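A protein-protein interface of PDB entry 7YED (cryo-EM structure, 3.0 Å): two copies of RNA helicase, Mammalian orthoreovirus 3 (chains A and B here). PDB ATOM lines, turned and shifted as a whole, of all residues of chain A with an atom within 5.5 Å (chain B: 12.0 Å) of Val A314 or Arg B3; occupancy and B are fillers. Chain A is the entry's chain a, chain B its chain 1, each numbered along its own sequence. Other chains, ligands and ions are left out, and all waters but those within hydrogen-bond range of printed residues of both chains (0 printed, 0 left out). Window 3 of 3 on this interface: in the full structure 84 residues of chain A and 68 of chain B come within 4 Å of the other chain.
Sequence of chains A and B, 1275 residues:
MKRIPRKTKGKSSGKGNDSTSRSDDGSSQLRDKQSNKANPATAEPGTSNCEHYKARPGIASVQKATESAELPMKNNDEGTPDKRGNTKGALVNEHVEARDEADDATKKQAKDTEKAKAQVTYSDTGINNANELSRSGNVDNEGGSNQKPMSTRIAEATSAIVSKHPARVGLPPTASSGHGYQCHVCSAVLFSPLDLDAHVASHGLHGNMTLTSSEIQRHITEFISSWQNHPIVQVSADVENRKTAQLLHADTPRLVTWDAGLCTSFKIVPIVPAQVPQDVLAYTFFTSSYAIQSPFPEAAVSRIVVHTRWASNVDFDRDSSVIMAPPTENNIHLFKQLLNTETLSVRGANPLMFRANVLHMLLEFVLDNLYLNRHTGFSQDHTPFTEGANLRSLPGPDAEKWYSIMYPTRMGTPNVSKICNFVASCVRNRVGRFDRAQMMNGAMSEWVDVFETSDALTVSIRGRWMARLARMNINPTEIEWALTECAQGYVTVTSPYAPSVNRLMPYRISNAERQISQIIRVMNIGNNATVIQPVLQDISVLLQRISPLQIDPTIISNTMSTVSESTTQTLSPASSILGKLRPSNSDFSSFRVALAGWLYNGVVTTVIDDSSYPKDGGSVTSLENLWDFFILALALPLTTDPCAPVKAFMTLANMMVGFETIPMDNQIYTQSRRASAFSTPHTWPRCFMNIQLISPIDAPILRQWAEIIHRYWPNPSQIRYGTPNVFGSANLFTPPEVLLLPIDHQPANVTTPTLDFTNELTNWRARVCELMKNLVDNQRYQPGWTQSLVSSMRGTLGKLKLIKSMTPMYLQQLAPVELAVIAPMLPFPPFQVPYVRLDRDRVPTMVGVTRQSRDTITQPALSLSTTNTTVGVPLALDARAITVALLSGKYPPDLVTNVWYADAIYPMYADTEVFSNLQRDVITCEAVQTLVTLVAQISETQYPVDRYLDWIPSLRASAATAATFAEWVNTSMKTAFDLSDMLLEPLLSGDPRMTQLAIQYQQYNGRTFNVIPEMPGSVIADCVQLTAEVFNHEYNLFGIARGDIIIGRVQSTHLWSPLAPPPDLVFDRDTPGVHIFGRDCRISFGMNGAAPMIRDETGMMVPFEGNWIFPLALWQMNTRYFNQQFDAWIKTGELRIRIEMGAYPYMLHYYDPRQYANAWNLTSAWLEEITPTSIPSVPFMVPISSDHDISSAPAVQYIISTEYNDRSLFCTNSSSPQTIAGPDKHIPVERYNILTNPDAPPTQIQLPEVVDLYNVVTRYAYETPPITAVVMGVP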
ATOM      1  N   TRP A 258       4.946  -1.324   9.414  1.00  0.00           N
ATOM      2  CA  TRP A 258       5.765  -2.482   9.743  1.00  0.00           C
ATOM      3  C   TRP A 258       6.524  -2.258  11.044  1.00  0.00           C
ATOM      4  O   TRP A 258       6.738  -1.123  11.469  1.00  0.00           O
ATOM      5  CB  TRP A 258       6.715  -2.806   8.607  1.00  0.00           C
ATOM      6  CG  TRP A 258       5.992  -3.275   7.409  1.00  0.00           C
ATOM      7  CD1 TRP A 258       5.478  -2.518   6.406  1.00  0.00           C
ATOM      8  CD2 TRP A 258       5.745  -4.638   7.041  1.00  0.00           C
ATOM      9  NE1 TRP A 258       4.882  -3.321   5.458  1.00  0.00           N
ATOM     10  CE2 TRP A 258       5.044  -4.626   5.821  1.00  0.00           C
ATOM     11  CE3 TRP A 258       6.044  -5.866   7.633  1.00  0.00           C
ATOM     12  CZ2 TRP A 258       4.646  -5.777   5.186  1.00  0.00           C
ATOM     13  CZ3 TRP A 258       5.649  -7.011   6.996  1.00  0.00           C
ATOM     14  CH2 TRP A 258       4.968  -6.966   5.788  1.00  0.00           C
ATOM     15  N   ASP A 259       6.990  -3.367  11.628  1.00  0.00           N
ATOM     16  CA  ASP A 259       7.693  -3.369  12.905  1.00  0.00           C
ATOM     17  C   ASP A 259       8.764  -4.444  12.865  1.00  0.00           C
ATOM     18  O   ASP A 259       8.528  -5.542  12.358  1.00  0.00           O
ATOM     19  CB  ASP A 259       6.737  -3.637  14.079  1.00  0.00           C
ATOM     20  CG  ASP A 259       7.402  -3.464  15.441  1.00  0.00           C
ATOM     21  OD1 ASP A 259       8.607  -3.161  15.488  1.00  0.00           O
ATOM     22  OD2 ASP A 259       6.712  -3.631  16.467  1.00  0.00           O
ATOM     23  N   ALA A 260       9.941  -4.126  13.400  1.00  0.00           N
ATOM     24  CA  ALA A 260      11.058  -5.057  13.410  1.00  0.00           C
ATOM     25  C   ALA A 260      11.557  -5.407  14.800  1.00  0.00           C
ATOM     26  O   ALA A 260      12.271  -6.404  14.943  1.00  0.00           O
ATOM     27  CB  ALA A 260      12.232  -4.498  12.594  1.00  0.00           C
ATOM     28  N   ARG A 309       5.020  -1.207  23.055  1.00  0.00           N
ATOM     29  CA  ARG A 309       6.111  -0.969  22.110  1.00  0.00           C
ATOM     30  C   ARG A 309       7.340  -0.385  22.798  1.00  0.00           C
ATOM     31  O   ARG A 309       7.863   0.657  22.404  1.00  0.00           O
ATOM     32  CB  ARG A 309       5.660  -0.064  20.964  1.00  0.00           C
ATOM     33  CG  ARG A 309       4.699  -0.706  20.005  1.00  0.00           C
ATOM     34  CD  ARG A 309       4.416   0.216  18.850  1.00  0.00           C
ATOM     35  NE  ARG A 309       3.674   1.398  19.263  1.00  0.00           N
ATOM     36  CZ  ARG A 309       4.155   2.634  19.209  1.00  0.00           C
ATOM     37  NH1 ARG A 309       5.380   2.848  18.754  1.00  0.00           N
ATOM     38  NH2 ARG A 309       3.411   3.654  19.609  1.00  0.00           N
ATOM     39  N   SER A 312      10.730  -1.745  19.852  1.00  0.00           N
ATOM     40  CA  SER A 312      10.032  -1.755  18.571  1.00  0.00           C
ATOM     41  C   SER A 312      10.690  -0.765  17.622  1.00  0.00           C
ATOM     42  O   SER A 312      10.654   0.443  17.869  1.00  0.00           O
ATOM     43  CB  SER A 312       8.563  -1.420  18.772  1.00  0.00           C
ATOM     44  OG  SER A 312       7.879  -1.385  17.537  1.00  0.00           O
ATOM     45  N   ASN A 313      11.277  -1.276  16.543  1.00  0.00           N
ATOM     46  CA  ASN A 313      11.723  -0.447  15.429  1.00  0.00           C
ATOM     47  C   ASN A 313      10.565  -0.318  14.454  1.00  0.00           C
ATOM     48  O   ASN A 313      10.157  -1.303  13.832  1.00  0.00           O
ATOM     49  CB  ASN A 313      12.943  -1.055  14.745  1.00  0.00           C
ATOM     50  CG  ASN A 313      14.191  -0.945  15.579  1.00  0.00           C
ATOM     51  OD1 ASN A 313      14.452   0.089  16.186  1.00  0.00           O
ATOM     52  ND2 ASN A 313      14.975  -2.012  15.613  1.00  0.00           N
ATOM     53  N   VAL A 314      10.031   0.888  14.318  1.00  0.00           N
ATOM     54  CA  VAL A 314       8.849   1.137  13.506  1.00  0.00           C
ATOM     55  C   VAL A 314       9.197   2.154  12.435  1.00  0.00           C
ATOM     56  O   VAL A 314       9.969   3.087  12.681  1.00  0.00           O
ATOM     57  CB  VAL A 314       7.679   1.640  14.370  1.00  0.00           C
ATOM     58  CG1 VAL A 314       6.482   1.950  13.506  1.00  0.00           C
ATOM     59  CG2 VAL A 314       7.328   0.614  15.413  1.00  0.00           C
ATOM     60  N   ASP A 315       8.629   1.979  11.245  1.00  0.00           N
ATOM     61  CA  ASP A 315       8.805   2.988  10.210  1.00  0.00           C
ATOM     62  C   ASP A 315       7.802   4.124  10.352  1.00  0.00           C
ATOM     63  O   ASP A 315       8.124   5.273  10.030  1.00  0.00           O
ATOM     64  CB  ASP A 315       8.697   2.355   8.826  1.00  0.00           C
ATOM     65  CG  ASP A 315       7.350   1.717   8.577  1.00  0.00           C
ATOM     66  OD1 ASP A 315       6.518   1.679   9.504  1.00  0.00           O
ATOM     67  OD2 ASP A 315       7.120   1.257   7.441  1.00  0.00           O
ATOM     68  N   PHE A 316       6.596   3.826  10.827  1.00  0.00           N
ATOM     69  CA  PHE A 316       5.554   4.827  11.019  1.00  0.00           C
ATOM     70  C   PHE A 316       4.805   4.489  12.295  1.00  0.00           C
ATOM     71  O   PHE A 316       4.162   3.439  12.369  1.00  0.00           O
ATOM     72  CB  PHE A 316       4.593   4.848   9.832  1.00  0.00           C
ATOM     73  CG  PHE A 316       3.496   5.854   9.962  1.00  0.00           C
ATOM     74  CD1 PHE A 316       3.725   7.186   9.691  1.00  0.00           C
ATOM     75  CD2 PHE A 316       2.234   5.468  10.361  1.00  0.00           C
ATOM     76  CE1 PHE A 316       2.714   8.107   9.807  1.00  0.00           C
ATOM     77  CE2 PHE A 316       1.222   6.386  10.479  1.00  0.00           C
ATOM     78  CZ  PHE A 316       1.461   7.707  10.203  1.00  0.00           C
ATOM     79  N   ASP A 317       4.873   5.363  13.295  1.00  0.00           N
ATOM     80  CA  ASP A 317       4.257   5.066  14.579  1.00  0.00           C
ATOM     81  C   ASP A 317       2.804   5.525  14.612  1.00  0.00           C
ATOM     82  O   ASP A 317       2.478   6.623  14.155  1.00  0.00           O
ATOM     83  CB  ASP A 317       5.036   5.692  15.735  1.00  0.00           C
ATOM     84  CG  ASP A 317       5.156   7.183  15.617  1.00  0.00           C
ATOM     85  OD1 ASP A 317       4.754   7.744  14.583  1.00  0.00           O
ATOM     86  OD2 ASP A 317       5.657   7.803  16.575  1.00  0.00           O
ATOM     87  N   TYR A 371       0.421  -3.054  13.939  1.00  0.00           N
ATOM     88  CA  TYR A 371       1.592  -3.091  13.083  1.00  0.00           C
ATOM     89  C   TYR A 371       1.673  -4.440  12.400  1.00  0.00           C
ATOM     90  O   TYR A 371       0.766  -5.268  12.490  1.00  0.00           O
ATOM     91  CB  TYR A 371       2.864  -2.800  13.871  1.00  0.00           C
ATOM     92  CG  TYR A 371       2.972  -1.374  14.297  1.00  0.00           C
ATOM     93  CD1 TYR A 371       2.153  -0.412  13.750  1.00  0.00           C
ATOM     94  CD2 TYR A 371       3.890  -0.986  15.243  1.00  0.00           C
ATOM     95  CE1 TYR A 371       2.245   0.886  14.133  1.00  0.00           C
ATOM     96  CE2 TYR A 371       3.986   0.315  15.630  1.00  0.00           C
ATOM     97  CZ  TYR A 371       3.159   1.245  15.076  1.00  0.00           C
ATOM     98  OH  TYR A 371       3.254   2.546  15.474  1.00  0.00           O
ATOM     99  N   LYS B   2      14.563   2.685   7.369  1.00  0.00           N
ATOM    100  CA  LYS B   2      13.508   3.453   6.724  1.00  0.00           C
ATOM    101  C   LYS B   2      12.670   4.183   7.762  1.00  0.00           C
ATOM    102  O   LYS B   2      12.434   3.665   8.852  1.00  0.00           O
ATOM    103  CB  LYS B   2      12.624   2.539   5.879  1.00  0.00           C
ATOM    104  CG  LYS B   2      11.863   1.514   6.699  1.00  0.00           C
ATOM    105  CD  LYS B   2      11.081   0.553   5.821  1.00  0.00           C
ATOM    106  CE  LYS B   2      10.286  -0.429   6.669  1.00  0.00           C
ATOM    107  NZ  LYS B   2      11.167  -1.338   7.456  1.00  0.00           N
ATOM    108  N   ARG B   3      12.228   5.392   7.425  1.00  0.00           N
ATOM    109  CA  ARG B   3      11.391   6.179   8.320  1.00  0.00           C
ATOM    110  C   ARG B   3      10.420   6.993   7.486  1.00  0.00           C
ATOM    111  O   ARG B   3      10.821   7.629   6.508  1.00  0.00           O
ATOM    112  CB  ARG B   3      12.230   7.103   9.206  1.00  0.00           C
ATOM    113  CG  ARG B   3      13.152   6.377  10.167  1.00  0.00           C
ATOM    114  CD  ARG B   3      12.369   5.659  11.249  1.00  0.00           C
ATOM    115  NE  ARG B   3      13.245   5.050  12.243  1.00  0.00           N
ATOM    116  CZ  ARG B   3      13.715   3.809  12.166  1.00  0.00           C
ATOM    117  NH1 ARG B   3      13.395   3.042  11.134  1.00  0.00           N
ATOM    118  NH2 ARG B   3      14.508   3.336  13.117  1.00  0.00           N
ATOM    119  N   ILE B   4       9.153   6.973   7.873  1.00  0.00           N
ATOM    120  CA  ILE B   4       8.090   7.690   7.181  1.00  0.00           C
ATOM    121  C   ILE B   4       7.608   8.808   8.095  1.00  0.00           C
ATOM    122  O   ILE B   4       7.096   8.529   9.187  1.00  0.00           O
ATOM    123  CB  ILE B   4       6.935   6.755   6.796  1.00  0.00           C
ATOM    124  CG1 ILE B   4       7.426   5.693   5.814  1.00  0.00           C
ATOM    125  CG2 ILE B   4       5.792   7.544   6.193  1.00  0.00           C
ATOM    126  CD1 ILE B   4       6.440   4.584   5.588  1.00  0.00           C
ATOM    127  N   PRO B   5       7.747  10.073   7.705  1.00  0.00           N
ATOM    128  CA  PRO B   5       7.371  11.166   8.607  1.00  0.00           C
ATOM    129  C   PRO B   5       5.862  11.249   8.785  1.00  0.00           C
ATOM    130  O   PRO B   5       5.108  11.287   7.811  1.00  0.00           O
ATOM    131  CB  PRO B   5       7.927  12.409   7.905  1.00  0.00           C
ATOM    132  CG  PRO B   5       7.959  12.032   6.467  1.00  0.00           C
ATOM    133  CD  PRO B   5       8.284  10.568   6.428  1.00  0.00           C
ATOM    134  N   ARG B   6       5.434  11.261  10.044  1.00  0.00           N
ATOM    135  CA  ARG B   6       4.040  11.515  10.376  1.00  0.00           C
ATOM    136  C   ARG B   6       3.597  12.844   9.781  1.00  0.00           C
ATOM    137  O   ARG B   6       4.391  13.776   9.637  1.00  0.00           O
ATOM    138  CB  ARG B   6       3.868  11.524  11.896  1.00  0.00           C
ATOM    139  CG  ARG B   6       2.466  11.792  12.389  1.00  0.00           C
ATOM    140  CD  ARG B   6       1.548  10.648  12.051  1.00  0.00           C
ATOM    141  NE  ARG B   6       0.199  10.870  12.556  1.00  0.00           N
ATOM    142  CZ  ARG B   6      -0.209  10.486  13.757  1.00  0.00           C
ATOM    143  NH1 ARG B   6       0.632   9.861  14.565  1.00  0.00           N
ATOM    144  NH2 ARG B   6      -1.454  10.720  14.148  1.00  0.00           N
ATOM    145  N   LYS B   7       2.316  12.934   9.424  1.00  0.00           N
ATOM    146  CA  LYS B   7       1.778  14.133   8.793  1.00  0.00           C
ATOM    147  C   LYS B   7       0.582  14.692   9.556  1.00  0.00           C
ATOM    148  O   LYS B   7      -0.270  15.368   8.979  1.00  0.00           O
ATOM    149  CB  LYS B   7       1.398  13.860   7.340  1.00  0.00           C
ATOM    150  CG  LYS B   7       0.237  12.906   7.179  1.00  0.00           C
ATOM    151  CD  LYS B   7      -0.068  12.668   5.716  1.00  0.00           C
ATOM    152  CE  LYS B   7      -0.653  13.913   5.079  1.00  0.00           C
ATOM    153  NZ  LYS B   7      -1.980  14.248   5.660  1.00  0.00           N
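N of Ile B4 is in hydrogen-bond range of O of Asp A315, at 2.9 Å.
The backbone NH (N) of Trp A258 is in hydrogen-bond range of the side-chain carboxylate (OD1) of Asp A315 (3.4 Å).
The side-chain hydroxyl (OH) of Tyr A371 sits at hydrogen-bond distance from the backbone carbonyl oxygen (O) of Phe A316 (3.4 Å).
Val A314 touches Arg B3.
OD2 of Asp A315 touches CE of Lys B2, 3.7 Å away.
Asp A315 touches Arg B3 (O to CA, 3.8 Å).
Phe A316 touches Ile B4.
Phe A316 touches Arg B6.
Asp A317 touches Arg B6.
Trp A258 touches none of the printed residues of chain B.
No residue of chain B comes within 4 Å of Asp A259.
No residue of chain B comes within 4 Å of Ala A260.
Ser A312 touches none of the printed residues of chain B.
No residue of chain B comes within 4 Å of Asn A313.
Of chain B, only Arg B3 (3.8 Å) comes within 4 Å of Val A314.
Of chain B, only Lys B2 (3.7 Å), Arg B3 (3.8 Å) and Ile B4 (2.9 Å) come within 4 Å of Asp A315.
Asp A317 touches just one residue of chain B: Arg B6.
Of chain A, only Val A314 and Asp A315 come within 4 Å of Arg B3.
Printed residues of chain A within 4 Å of Ile B4: Asp A315 (2.9 Å) and Phe A316 (3.7 Å).
Of the printed residues of chain A, Arg B6 touches Phe A316 (3.5 Å) and Asp A317 (3.7 Å).
The nearest printed residue of chain A that does not touch Lys B2 is Val A314 (4.6 Å).
Hydrophobic or aromatic side chains of chain B that line the printed part of chain A: Ile B4.
Hydrophobic or aromatic side chains of chain A within 4 Å of the printed part of chain B: Phe A316.
Along chain A the printed residues that touch a printed residue of chain B span positions 314 to 317.
Among the printed residues, no Asp or Glu carboxylate lies within 4 Å of a Lys or Arg side-chain nitrogen of the other chain.
No position is printed for both chains.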
